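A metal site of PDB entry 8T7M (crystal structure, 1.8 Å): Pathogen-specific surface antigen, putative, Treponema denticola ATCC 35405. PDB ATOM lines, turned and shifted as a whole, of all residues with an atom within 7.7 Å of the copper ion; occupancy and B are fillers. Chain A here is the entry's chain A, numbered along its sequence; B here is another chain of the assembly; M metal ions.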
ATOM      1  N   PHE A  26       4.295   1.873   8.084  1.00  0.00           N
ATOM      2  CA  PHE A  26       5.277   0.891   7.623  1.00  0.00           C
ATOM      3  C   PHE A  26       6.461   1.674   7.057  1.00  0.00           C
ATOM      4  O   PHE A  26       6.539   2.895   7.212  1.00  0.00           O
ATOM      5  CB  PHE A  26       4.648  -0.092   6.625  1.00  0.00           C
ATOM      6  CG  PHE A  26       3.821   0.548   5.533  1.00  0.00           C
ATOM      7  CD1 PHE A  26       4.425   0.963   4.353  1.00  0.00           C
ATOM      8  CD2 PHE A  26       2.450   0.713   5.684  1.00  0.00           C
ATOM      9  CE1 PHE A  26       3.660   1.532   3.337  1.00  0.00           C
ATOM     10  CE2 PHE A  26       1.691   1.290   4.666  1.00  0.00           C
ATOM     11  CZ  PHE A  26       2.297   1.691   3.489  1.00  0.00           C
ATOM     12  N   VAL A  29       8.396   5.023   1.540  1.00  0.00           N
ATOM     13  CA  VAL A  29       8.221   4.543   0.171  1.00  0.00           C
ATOM     14  C   VAL A  29       8.643   5.616  -0.830  1.00  0.00           C
ATOM     15  O   VAL A  29       8.876   6.778  -0.472  1.00  0.00           O
ATOM     16  CB  VAL A  29       6.750   4.135  -0.111  1.00  0.00           C
ATOM     17  CG1 VAL A  29       6.276   3.112   0.911  1.00  0.00           C
ATOM     18  CG2 VAL A  29       5.863   5.361  -0.116  1.00  0.00           C
ATOM     19  N   ASP A  30       8.702   5.219  -2.107  1.00  0.00           N
ATOM     20  CA  ASP A  30       8.944   6.147  -3.207  1.00  0.00           C
ATOM     21  C   ASP A  30       7.624   6.415  -3.917  1.00  0.00           C
ATOM     22  O   ASP A  30       6.901   5.481  -4.264  1.00  0.00           O
ATOM     23  CB  ASP A  30       9.947   5.590  -4.235  1.00  0.00           C
ATOM     24  CG  ASP A  30      11.355   5.425  -3.657  1.00  0.00           C
ATOM     25  OD1 ASP A  30      11.895   6.386  -3.050  1.00  0.00           O
ATOM     26  OD2 ASP A  30      11.930   4.332  -3.875  1.00  0.00           O
ATOM     27  N   MET A  31       7.308   7.690  -4.127  1.00  0.00           N
ATOM     28  CA  MET A  31       6.065   8.082  -4.777  1.00  0.00           C
ATOM     29  C   MET A  31       6.349   8.760  -6.119  1.00  0.00           C
ATOM     30  O   MET A  31       7.310   9.523  -6.237  1.00  0.00           O
ATOM     31  CB  MET A  31       5.263   9.015  -3.861  1.00  0.00           C
ATOM     32  CG  MET A  31       4.599   8.295  -2.707  1.00  0.00           C
ATOM     33  SD  MET A  31       4.200   9.338  -1.291  1.00  0.00           S
ATOM     34  CE  MET A  31       5.814   9.620  -0.553  1.00  0.00           C
ATOM     35  N   HIS A  46       6.205   5.498   6.353  1.00  0.00           N
ATOM     36  CA  HIS A  46       5.050   5.910   5.559  1.00  0.00           C
ATOM     37  C   HIS A  46       3.846   5.795   6.491  1.00  0.00           C
ATOM     38  O   HIS A  46       3.718   4.799   7.221  1.00  0.00           O
ATOM     39  CB  HIS A  46       4.864   5.037   4.327  1.00  0.00           C
ATOM     40  CG  HIS A  46       3.896   5.599   3.343  1.00  0.00           C
ATOM     41  ND1 HIS A  46       4.145   6.748   2.621  1.00  0.00           N
ATOM     42  CD2 HIS A  46       2.639   5.206   2.996  1.00  0.00           C
ATOM     43  CE1 HIS A  46       3.111   7.023   1.844  1.00  0.00           C
ATOM     44  NE2 HIS A  46       2.178   6.104   2.060  1.00  0.00           N
ATOM     45  N   MET A  47       2.994   6.812   6.515  1.00  0.00           N
ATOM     46  CA  MET A  47       1.809   6.803   7.358  1.00  0.00           C
ATOM     47  C   MET A  47       0.582   6.910   6.456  1.00  0.00           C
ATOM     48  O   MET A  47       0.593   7.670   5.489  1.00  0.00           O
ATOM     49  CB  MET A  47       1.834   7.951   8.377  1.00  0.00           C
ATOM     50  CG  MET A  47       0.691   7.925   9.378  1.00  0.00           C
ATOM     51  SD  MET A  47       0.924   9.088  10.733  1.00  0.00           S
ATOM     52  CE  MET A  47       2.455   8.494  11.480  1.00  0.00           C
ATOM     53  N   GLU A  48      -0.459   6.147   6.763  1.00  0.00           N
ATOM     54  CA  GLU A  48      -1.627   6.171   5.878  1.00  0.00           C
ATOM     55  C   GLU A  48      -2.927   6.137   6.671  1.00  0.00           C
ATOM     56  O   GLU A  48      -3.004   5.579   7.778  1.00  0.00           O
ATOM     57  CB  GLU A  48      -1.538   5.021   4.864  1.00  0.00           C
ATOM     58  CG  GLU A  48      -2.361   3.801   5.147  1.00  0.00           C
ATOM     59  CD  GLU A  48      -2.037   2.677   4.166  1.00  0.00           C
ATOM     60  OE1 GLU A  48      -1.233   2.886   3.231  1.00  0.00           O
ATOM     61  OE2 GLU A  48      -2.601   1.582   4.335  1.00  0.00           O
ATOM     62  N   ALA A  49      -3.933   6.827   6.122  1.00  0.00           N
ATOM     63  CA  ALA A  49      -5.318   6.733   6.543  1.00  0.00           C
ATOM     64  C   ALA A  49      -6.067   5.873   5.531  1.00  0.00           C
ATOM     65  O   ALA A  49      -6.192   6.265   4.372  1.00  0.00           O
ATOM     66  CB  ALA A  49      -5.950   8.117   6.632  1.00  0.00           C
ATOM     67  N   MET A  91      -1.783  12.718   0.878  1.00  0.00           N
ATOM     68  CA  MET A  91      -2.213  12.751  -0.520  1.00  0.00           C
ATOM     69  C   MET A  91      -2.917  11.455  -0.862  1.00  0.00           C
ATOM     70  O   MET A  91      -2.576  10.398  -0.326  1.00  0.00           O
ATOM     71  CB  MET A  91      -1.041  12.948  -1.490  1.00  0.00           C
ATOM     72  CG  MET A  91      -0.626  14.394  -1.622  1.00  0.00           C
ATOM     73  SD  MET A  91      -1.640  15.297  -2.810  1.00  0.00           S
ATOM     74  CE  MET A  91      -1.495  14.305  -4.328  1.00  0.00           C
ATOM     75  N   PRO A  92      -3.862  11.492  -1.793  1.00  0.00           N
ATOM     76  CA  PRO A  92      -4.457  10.228  -2.262  1.00  0.00           C
ATOM     77  C   PRO A  92      -3.480   9.542  -3.205  1.00  0.00           C
ATOM     78  O   PRO A  92      -2.789  10.185  -3.982  1.00  0.00           O
ATOM     79  CB  PRO A  92      -5.733  10.693  -2.991  1.00  0.00           C
ATOM     80  CG  PRO A  92      -5.380  12.062  -3.482  1.00  0.00           C
ATOM     81  CD  PRO A  92      -4.557  12.666  -2.350  1.00  0.00           C
ATOM     82  N   MET A  93      -3.416   8.223  -3.096  1.00  0.00           N
ATOM     83  CA  MET A  93      -2.435   7.474  -3.871  1.00  0.00           C
ATOM     84  C   MET A  93      -2.789   5.990  -3.835  1.00  0.00           C
ATOM     85  O   MET A  93      -3.580   5.552  -3.011  1.00  0.00           O
ATOM     86  CB  MET A  93      -1.021   7.678  -3.341  1.00  0.00           C
ATOM     87  CG  MET A  93      -0.812   7.010  -1.965  1.00  0.00           C
ATOM     88  SD  MET A  93       0.754   7.463  -1.194  1.00  0.00           S
ATOM     89  CE  MET A  93       0.636   9.254  -1.166  1.00  0.00           C
ATOM     90  N   ASN A  94      -2.188   5.237  -4.765  1.00  0.00           N
ATOM     91  CA  ASN A  94      -2.264   3.786  -4.782  1.00  0.00           C
ATOM     92  C   ASN A  94      -0.928   3.195  -4.366  1.00  0.00           C
ATOM     93  O   ASN A  94       0.124   3.639  -4.823  1.00  0.00           O
ATOM     94  CB  ASN A  94      -2.581   3.265  -6.196  1.00  0.00           C
ATOM     95  CG  ASN A  94      -4.052   3.120  -6.448  1.00  0.00           C
ATOM     96  OD1 ASN A  94      -4.883   3.380  -5.584  1.00  0.00           O
ATOM     97  ND2 ASN A  94      -4.396   2.725  -7.685  1.00  0.00           N
ATOM     98  N   ALA A  95      -0.987   2.180  -3.500  1.00  0.00           N
ATOM     99  CA  ALA A  95       0.064   1.198  -3.284  1.00  0.00           C
ATOM    100  C   ALA A  95      -0.400  -0.123  -3.901  1.00  0.00           C
ATOM    101  O   ALA A  95      -1.471  -0.185  -4.512  1.00  0.00           O
ATOM    102  CB  ALA A  95       0.391   1.051  -1.792  1.00  0.00           C
ATOM    103  N   ASP A  97      -1.615  -2.526  -2.448  1.00  0.00           N
ATOM    104  CA  ASP A  97      -2.790  -2.961  -1.708  1.00  0.00           C
ATOM    105  C   ASP A  97      -3.985  -2.023  -1.895  1.00  0.00           C
ATOM    106  O   ASP A  97      -5.003  -2.190  -1.208  1.00  0.00           O
ATOM    107  CB  ASP A  97      -2.461  -3.072  -0.225  1.00  0.00           C
ATOM    108  CG  ASP A  97      -2.315  -1.723   0.442  1.00  0.00           C
ATOM    109  OD1 ASP A  97      -1.724  -0.803  -0.170  1.00  0.00           O
ATOM    110  OD2 ASP A  97      -2.765  -1.581   1.593  1.00  0.00           O
ATOM    111  N   GLY A  98      -3.874  -1.022  -2.750  1.00  0.00           N
ATOM    112  CA  GLY A  98      -5.013  -0.206  -3.107  1.00  0.00           C
ATOM    113  C   GLY A  98      -4.924   1.250  -2.700  1.00  0.00           C
ATOM    114  O   GLY A  98      -3.882   1.732  -2.250  1.00  0.00           O
ATOM    115  N   PRO A  99      -6.020   1.976  -2.872  1.00  0.00           N
ATOM    116  CA  PRO A  99      -6.017   3.415  -2.591  1.00  0.00           C
ATOM    117  C   PRO A  99      -6.051   3.704  -1.104  1.00  0.00           C
ATOM    118  O   PRO A  99      -6.579   2.930  -0.304  1.00  0.00           O
ATOM    119  CB  PRO A  99      -7.286   3.913  -3.277  1.00  0.00           C
ATOM    120  CG  PRO A  99      -8.199   2.734  -3.215  1.00  0.00           C
ATOM    121  CD  PRO A  99      -7.315   1.529  -3.432  1.00  0.00           C
ATOM    122  N   HIS A 100      -5.474   4.846  -0.739  1.00  0.00           N
ATOM    123  CA  HIS A 100      -5.419   5.322   0.637  1.00  0.00           C
ATOM    124  C   HIS A 100      -4.980   6.781   0.583  1.00  0.00           C
ATOM    125  O   HIS A 100      -4.603   7.286  -0.484  1.00  0.00           O
ATOM    126  CB  HIS A 100      -4.464   4.478   1.483  1.00  0.00           C
ATOM    127  CG  HIS A 100      -3.040   4.497   1.007  1.00  0.00           C
ATOM    128  ND1 HIS A 100      -2.555   3.602   0.086  1.00  0.00           N
ATOM    129  CD2 HIS A 100      -1.998   5.283   1.353  1.00  0.00           C
ATOM    130  CE1 HIS A 100      -1.277   3.854  -0.141  1.00  0.00           C
ATOM    131  NE2 HIS A 100      -0.907   4.860   0.639  1.00  0.00           N
ATOM    132  N   TYR A 101      -5.009   7.448   1.721  1.00  0.00           N
ATOM    133  CA  TYR A 101      -4.376   8.750   1.870  1.00  0.00           C
ATOM    134  C   TYR A 101      -3.104   8.536   2.672  1.00  0.00           C
ATOM    135  O   TYR A 101      -3.123   7.821   3.680  1.00  0.00           O
ATOM    136  CB  TYR A 101      -5.285   9.756   2.589  1.00  0.00           C
ATOM    137  CG  TYR A 101      -6.585  10.032   1.876  1.00  0.00           C
ATOM    138  CD1 TYR A 101      -7.679   9.191   2.030  1.00  0.00           C
ATOM    139  CD2 TYR A 101      -6.717  11.136   1.040  1.00  0.00           C
ATOM    140  CE1 TYR A 101      -8.897   9.449   1.359  1.00  0.00           C
ATOM    141  CE2 TYR A 101      -7.914  11.403   0.365  1.00  0.00           C
ATOM    142  CZ  TYR A 101      -9.006  10.552   0.542  1.00  0.00           C
ATOM    143  OH  TYR A 101     -10.189  10.821  -0.134  1.00  0.00           O
ATOM    144  N   GLY A 102      -1.994   9.134   2.226  1.00  0.00           N
ATOM    145  CA  GLY A 102      -0.746   8.870   2.918  1.00  0.00           C
ATOM    146  C   GLY A 102       0.309   9.924   2.694  1.00  0.00           C
ATOM    147  O   GLY A 102       0.169  10.829   1.886  1.00  0.00           O
ATOM    148  N   ALA A 103       1.389   9.771   3.471  1.00  0.00           N
ATOM    149  CA  ALA A 103       2.579  10.589   3.328  1.00  0.00           C
ATOM    150  C   ALA A 103       3.739   9.871   4.000  1.00  0.00           C
ATOM    151  O   ALA A 103       3.542   9.102   4.947  1.00  0.00           O
ATOM    152  CB  ALA A 103       2.405  11.982   3.958  1.00  0.00           C
ATOM    153  N   ASN A 104       4.948  10.117   3.499  1.00  0.00           N
ATOM    154  CA  ASN A 104       6.141   9.797   4.259  1.00  0.00           C
ATOM    155  C   ASN A 104       6.240  10.747   5.457  1.00  0.00           C
ATOM    156  O   ASN A 104       5.972  11.951   5.324  1.00  0.00           O
ATOM    157  CB  ASN A 104       7.389   9.941   3.370  1.00  0.00           C
ATOM    158  CG  ASN A 104       7.612   8.739   2.475  1.00  0.00           C
ATOM    159  OD1 ASN A 104       6.987   7.680   2.637  1.00  0.00           O
ATOM    160  ND2 ASN A 104       8.502   8.901   1.485  1.00  0.00           N
ATOM    161  N   LEU B 128      -0.951   9.967  -6.523  1.00  0.00           N
ATOM    162  CA  LEU B 128       0.397   9.415  -6.600  1.00  0.00           C
ATOM    163  C   LEU B 128       0.321   7.901  -6.695  1.00  0.00           C
ATOM    164  O   LEU B 128      -0.714   7.282  -6.433  1.00  0.00           O
ATOM    165  CB  LEU B 128       1.216   9.823  -5.369  1.00  0.00           C
ATOM    166  CG  LEU B 128       1.110  11.271  -4.910  1.00  0.00           C
ATOM    167  CD1 LEU B 128       1.996  11.505  -3.672  1.00  0.00           C
ATOM    168  CD2 LEU B 128       1.424  12.270  -6.021  1.00  0.00           C
ATOM    169  N   LEU B 129       1.459   7.310  -7.062  1.00  0.00           N
ATOM    170  CA  LEU B 129       1.646   5.864  -7.083  1.00  0.00           C
ATOM    171  C   LEU B 129       2.882   5.526  -6.259  1.00  0.00           C
ATOM    172  O   LEU B 129       3.901   6.218  -6.363  1.00  0.00           O
ATOM    173  CB  LEU B 129       1.881   5.368  -8.520  1.00  0.00           C
ATOM    174  CG  LEU B 129       0.686   5.375  -9.492  1.00  0.00           C
ATOM    175  CD1 LEU B 129       1.116   4.813 -10.861  1.00  0.00           C
ATOM    176  CD2 LEU B 129      -0.485   4.609  -8.920  1.00  0.00           C
ATOM    177  N   HIS B 130       2.794   4.484  -5.437  1.00  0.00           N
ATOM    178  CA  HIS B 130       4.018   3.929  -4.849  1.00  0.00           C
ATOM    179  C   HIS B 130       4.771   3.219  -5.972  1.00  0.00           C
ATOM    180  O   HIS B 130       4.190   2.398  -6.682  1.00  0.00           O
ATOM    181  CB  HIS B 130       3.742   2.917  -3.716  1.00  0.00           C
ATOM    182  CG  HIS B 130       3.167   3.502  -2.459  1.00  0.00           C
ATOM    183  ND1 HIS B 130       3.151   2.811  -1.262  1.00  0.00           N
ATOM    184  CD2 HIS B 130       2.516   4.666  -2.213  1.00  0.00           C
ATOM    185  CE1 HIS B 130       2.568   3.538  -0.327  1.00  0.00           C
ATOM    186  NE2 HIS B 130       2.169   4.680  -0.881  1.00  0.00           N
ATOM    187  N   THR B 135       6.456  -1.974  -1.754  1.00  0.00           N
ATOM    188  CA  THR B 135       5.038  -1.631  -1.633  1.00  0.00           C
ATOM    189  C   THR B 135       4.409  -1.135  -2.926  1.00  0.00           C
ATOM    190  O   THR B 135       3.192  -0.905  -2.942  1.00  0.00           O
ATOM    191  CB  THR B 135       4.832  -0.552  -0.555  1.00  0.00           C
ATOM    192  OG1 THR B 135       5.233   0.727  -1.078  1.00  0.00           O
ATOM    193  CG2 THR B 135       5.614  -0.878   0.711  1.00  0.00           C
HETATM  194 CU    CU M   1       0.953   5.881   0.372  1.00  0.00          CU
HETATM  195 FE    FE M   2      -2.386  -0.013   3.019  1.00  0.00          FE
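OE1 of Glu 48 sits close to ND1 of His 100 (3.5 Å).
ND1 of His 100 is in hydrogen-bond range of O of Gly 98, at 3.3 Å.
A ring nitrogen (ND1) of His 46 lies within hydrogen-bond range of the side-chain amide oxygen (OD1) of Asn 104, 3.0 Å away.
OG1 of Thr 135 of chain B lies within hydrogen-bond range of ND1 of His 130 of chain B.
The backbone carbonyl oxygen (O) of Phe 26 sits at hydrogen-bond distance from the backbone NH (N) of His 46 (2.8 Å).
ND1 of His 46 lies within hydrogen-bond range of O of Ala 103, 3.4 Å away.
O of Asn 94 is in hydrogen-bond range of N of His 130 of chain B (2.9 Å).
The copper ion is bound by NE2 of His 46 (2.1 Å), NE2 of His 130 of chain B (2.1 Å), NE2 of His 100 (2.1 Å) and SD of Met 93 (2.2 Å).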
